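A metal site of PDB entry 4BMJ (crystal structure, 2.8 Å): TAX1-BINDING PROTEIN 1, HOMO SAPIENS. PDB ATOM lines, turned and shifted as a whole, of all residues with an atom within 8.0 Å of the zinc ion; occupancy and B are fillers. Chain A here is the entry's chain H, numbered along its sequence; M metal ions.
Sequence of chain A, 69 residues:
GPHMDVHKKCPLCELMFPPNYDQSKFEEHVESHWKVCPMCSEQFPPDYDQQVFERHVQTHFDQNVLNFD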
ATOM      1  N   LYS A   9      31.579 -20.316  -1.631  1.00  0.00           N
ATOM      2  CA  LYS A   9      30.677 -21.110  -0.819  1.00  0.00           C
ATOM      3  C   LYS A   9      29.798 -20.175  -0.004  1.00  0.00           C
ATOM      4  O   LYS A   9      30.242 -19.135   0.431  1.00  0.00           O
ATOM      5  CB  LYS A   9      31.416 -22.082   0.104  1.00  0.00           C
ATOM      6  CG  LYS A   9      30.503 -22.808   1.112  1.00  0.00           C
ATOM      7  CD  LYS A   9      31.166 -24.063   1.670  1.00  0.00           C
ATOM      8  CE  LYS A   9      32.630 -23.797   2.075  1.00  0.00           C
ATOM      9  NZ  LYS A   9      33.470 -25.034   2.182  1.00  0.00           N
ATOM     10  N   CYS A  10      28.540 -20.562   0.168  1.00  0.00           N
ATOM     11  CA  CYS A  10      27.638 -19.833   1.018  1.00  0.00           C
ATOM     12  C   CYS A  10      27.967 -20.103   2.472  1.00  0.00           C
ATOM     13  O   CYS A  10      28.124 -21.247   2.891  1.00  0.00           O
ATOM     14  CB  CYS A  10      26.190 -20.248   0.740  1.00  0.00           C
ATOM     15  SG  CYS A  10      24.950 -19.342   1.713  1.00  0.00           S
ATOM     16  N   PRO A  11      28.080 -19.042   3.260  1.00  0.00           N
ATOM     17  CA  PRO A  11      28.216 -19.118   4.704  1.00  0.00           C
ATOM     18  C   PRO A  11      27.125 -19.977   5.308  1.00  0.00           C
ATOM     19  O   PRO A  11      27.397 -20.825   6.146  1.00  0.00           O
ATOM     20  CB  PRO A  11      27.983 -17.675   5.152  1.00  0.00           C
ATOM     21  CG  PRO A  11      27.277 -17.012   3.972  1.00  0.00           C
ATOM     22  CD  PRO A  11      27.924 -17.649   2.792  1.00  0.00           C
ATOM     23  N   LEU A  12      25.886 -19.772   4.855  1.00  0.00           N
ATOM     24  CA  LEU A  12      24.736 -20.355   5.558  1.00  0.00           C
ATOM     25  C   LEU A  12      24.276 -21.695   5.016  1.00  0.00           C
ATOM     26  O   LEU A  12      23.843 -22.555   5.769  1.00  0.00           O
ATOM     27  CB  LEU A  12      23.575 -19.356   5.657  1.00  0.00           C
ATOM     28  CG  LEU A  12      24.023 -18.204   6.573  1.00  0.00           C
ATOM     29  CD1 LEU A  12      23.066 -17.007   6.580  1.00  0.00           C
ATOM     30  CD2 LEU A  12      24.300 -18.707   7.988  1.00  0.00           C
ATOM     31  N   CYS A  13      24.391 -21.912   3.716  1.00  0.00           N
ATOM     32  CA  CYS A  13      24.146 -23.249   3.240  1.00  0.00           C
ATOM     33  C   CYS A  13      25.372 -23.871   2.561  1.00  0.00           C
ATOM     34  O   CYS A  13      26.505 -23.538   2.879  1.00  0.00           O
ATOM     35  CB  CYS A  13      22.919 -23.285   2.350  1.00  0.00           C
ATOM     36  SG  CYS A  13      23.156 -22.418   0.830  1.00  0.00           S
ATOM     37  N   GLU A  14      25.113 -24.763   1.614  1.00  0.00           N
ATOM     38  CA  GLU A  14      26.139 -25.585   1.002  1.00  0.00           C
ATOM     39  C   GLU A  14      26.378 -25.189  -0.439  1.00  0.00           C
ATOM     40  O   GLU A  14      27.305 -25.651  -1.078  1.00  0.00           O
ATOM     41  CB  GLU A  14      25.673 -27.036   1.016  1.00  0.00           C
ATOM     42  CG  GLU A  14      26.773 -28.046   1.123  1.00  0.00           C
ATOM     43  CD  GLU A  14      27.418 -27.997   2.481  1.00  0.00           C
ATOM     44  OE1 GLU A  14      27.021 -27.134   3.285  1.00  0.00           O
ATOM     45  OE2 GLU A  14      28.324 -28.818   2.732  1.00  0.00           O
ATOM     46  N   LEU A  15      25.493 -24.365  -0.972  1.00  0.00           N
ATOM     47  CA  LEU A  15      25.598 -23.998  -2.367  1.00  0.00           C
ATOM     48  C   LEU A  15      26.899 -23.272  -2.678  1.00  0.00           C
ATOM     49  O   LEU A  15      27.510 -22.651  -1.802  1.00  0.00           O
ATOM     50  CB  LEU A  15      24.401 -23.132  -2.806  1.00  0.00           C
ATOM     51  CG  LEU A  15      23.230 -23.814  -3.520  1.00  0.00           C
ATOM     52  CD1 LEU A  15      23.618 -25.190  -4.021  1.00  0.00           C
ATOM     53  CD2 LEU A  15      22.025 -23.894  -2.600  1.00  0.00           C
ATOM     54  N   MET A  16      27.313 -23.342  -3.934  1.00  0.00           N
ATOM     55  CA  MET A  16      28.532 -22.679  -4.388  1.00  0.00           C
ATOM     56  C   MET A  16      28.207 -21.893  -5.663  1.00  0.00           C
ATOM     57  O   MET A  16      27.340 -22.287  -6.423  1.00  0.00           O
ATOM     58  CB  MET A  16      29.626 -23.719  -4.614  1.00  0.00           C
ATOM     59  CG  MET A  16      29.710 -24.694  -3.468  1.00  0.00           C
ATOM     60  SD  MET A  16      31.408 -25.006  -2.957  1.00  0.00           S
ATOM     61  CE  MET A  16      31.197 -25.947  -1.442  1.00  0.00           C
ATOM     62  N   PHE A  17      28.876 -20.769  -5.880  1.00  0.00           N
ATOM     63  CA  PHE A  17      28.519 -19.902  -7.003  1.00  0.00           C
ATOM     64  C   PHE A  17      29.675 -19.580  -7.928  1.00  0.00           C
ATOM     65  O   PHE A  17      30.780 -19.289  -7.463  1.00  0.00           O
ATOM     66  CB  PHE A  17      27.871 -18.612  -6.500  1.00  0.00           C
ATOM     67  CG  PHE A  17      26.653 -18.857  -5.662  1.00  0.00           C
ATOM     68  CD1 PHE A  17      26.776 -19.299  -4.366  1.00  0.00           C
ATOM     69  CD2 PHE A  17      25.377 -18.684  -6.192  1.00  0.00           C
ATOM     70  CE1 PHE A  17      25.668 -19.546  -3.588  1.00  0.00           C
ATOM     71  CE2 PHE A  17      24.251 -18.916  -5.421  1.00  0.00           C
ATOM     72  CZ  PHE A  17      24.394 -19.356  -4.119  1.00  0.00           C
ATOM     73  N   PHE A  26      23.827 -12.845  -5.027  1.00  0.00           N
ATOM     74  CA  PHE A  26      24.427 -13.685  -4.008  1.00  0.00           C
ATOM     75  C   PHE A  26      24.006 -13.240  -2.603  1.00  0.00           C
ATOM     76  O   PHE A  26      23.725 -14.078  -1.727  1.00  0.00           O
ATOM     77  CB  PHE A  26      25.936 -13.682  -4.130  1.00  0.00           C
ATOM     78  CG  PHE A  26      26.616 -14.355  -2.986  1.00  0.00           C
ATOM     79  CD1 PHE A  26      26.723 -15.735  -2.956  1.00  0.00           C
ATOM     80  CD2 PHE A  26      27.125 -13.623  -1.945  1.00  0.00           C
ATOM     81  CE1 PHE A  26      27.351 -16.374  -1.912  1.00  0.00           C
ATOM     82  CE2 PHE A  26      27.763 -14.252  -0.905  1.00  0.00           C
ATOM     83  CZ  PHE A  26      27.865 -15.632  -0.888  1.00  0.00           C
ATOM     84  N   HIS A  29      20.594 -14.340  -2.008  1.00  0.00           N
ATOM     85  CA  HIS A  29      20.502 -15.762  -1.656  1.00  0.00           C
ATOM     86  C   HIS A  29      20.690 -15.933  -0.174  1.00  0.00           C
ATOM     87  O   HIS A  29      19.898 -16.568   0.499  1.00  0.00           O
ATOM     88  CB  HIS A  29      21.542 -16.631  -2.367  1.00  0.00           C
ATOM     89  CG  HIS A  29      21.751 -17.986  -1.729  1.00  0.00           C
ATOM     90  ND1 HIS A  29      20.965 -19.088  -2.021  1.00  0.00           N
ATOM     91  CD2 HIS A  29      22.662 -18.412  -0.808  1.00  0.00           C
ATOM     92  CE1 HIS A  29      21.386 -20.129  -1.316  1.00  0.00           C
ATOM     93  NE2 HIS A  29      22.406 -19.743  -0.571  1.00  0.00           N
ATOM     94  N   VAL A  30      21.782 -15.398   0.332  1.00  0.00           N
ATOM     95  CA  VAL A  30      22.047 -15.631   1.721  1.00  0.00           C
ATOM     96  C   VAL A  30      20.897 -15.080   2.543  1.00  0.00           C
ATOM     97  O   VAL A  30      20.486 -15.712   3.529  1.00  0.00           O
ATOM     98  CB  VAL A  30      23.331 -14.983   2.176  1.00  0.00           C
ATOM     99  CG1 VAL A  30      23.620 -15.395   3.605  1.00  0.00           C
ATOM    100  CG2 VAL A  30      24.460 -15.389   1.260  1.00  0.00           C
ATOM    101  N   GLU A  31      20.377 -13.923   2.139  1.00  0.00           N
ATOM    102  CA  GLU A  31      19.271 -13.312   2.877  1.00  0.00           C
ATOM    103  C   GLU A  31      18.127 -14.304   3.012  1.00  0.00           C
ATOM    104  O   GLU A  31      17.444 -14.323   4.037  1.00  0.00           O
ATOM    105  CB  GLU A  31      18.756 -12.025   2.230  1.00  0.00           C
ATOM    106  CG  GLU A  31      17.414 -11.564   2.792  1.00  0.00           C
ATOM    107  CD  GLU A  31      16.858 -10.363   2.046  1.00  0.00           C
ATOM    108  OE1 GLU A  31      16.649 -10.466   0.809  1.00  0.00           O
ATOM    109  OE2 GLU A  31      16.607  -9.314   2.689  1.00  0.00           O
ATOM    110  N   SER A  32      17.931 -15.138   1.996  1.00  0.00           N
ATOM    111  CA  SER A  32      16.806 -16.023   1.973  1.00  0.00           C
ATOM    112  C   SER A  32      16.935 -17.211   2.936  1.00  0.00           C
ATOM    113  O   SER A  32      16.059 -18.069   2.967  1.00  0.00           O
ATOM    114  CB  SER A  32      16.568 -16.526   0.563  1.00  0.00           C
ATOM    115  OG  SER A  32      17.460 -17.595   0.258  1.00  0.00           O
ATOM    116  N   HIS A  33      18.003 -17.276   3.712  1.00  0.00           N
ATOM    117  CA  HIS A  33      18.064 -18.285   4.782  1.00  0.00           C
ATOM    118  C   HIS A  33      17.579 -17.681   6.102  1.00  0.00           C
ATOM    119  O   HIS A  33      17.175 -18.399   6.999  1.00  0.00           O
ATOM    120  CB  HIS A  33      19.498 -18.770   5.036  1.00  0.00           C
ATOM    121  CG  HIS A  33      20.140 -19.498   3.894  1.00  0.00           C
ATOM    122  ND1 HIS A  33      19.945 -20.840   3.657  1.00  0.00           N
ATOM    123  CD2 HIS A  33      21.075 -19.094   2.990  1.00  0.00           C
ATOM    124  CE1 HIS A  33      20.695 -21.218   2.640  1.00  0.00           C
ATOM    125  NE2 HIS A  33      21.396 -20.183   2.219  1.00  0.00           N
HETATM  126 ZN    ZN M   1      22.930 -20.567   1.126  1.00  0.00          ZN
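The zinc ion is bound by the side-chain sulfur of Cys 13 (1.9 Å), a ring nitrogen (NE2) of His 33 (1.9 Å), a ring nitrogen (NE2) of His 29 (2.0 Å) and the side-chain sulfur of Cys 10 (2.4 Å).
The zinc ion has four donor atoms within binding distance.
Four residues have an atom within 4 Å of the zinc ion: Cys 10, Cys 13, His 29 and His 33.
Along chain A the residues within 4 Å of the zinc ion span positions 10 to 33.
The nearest printed residue that does not touch the zinc ion is Leu 12 (4.3 Å).
The backbone carbonyl oxygen (O) of Leu 15 is in hydrogen-bond range of the backbone NH (N) of Cys 10, 3.1 Å away.
SG of Cys 13 lies close to N of Leu 15, 3.5 Å away.
The side-chain sulfur (SG) of Cys 10 sits close to the backbone NH (N) of Leu 12.
The backbone carbonyl oxygen of His 29 is in hydrogen-bond range of the side-chain hydroxyl of Ser 32 (2.7 Å).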
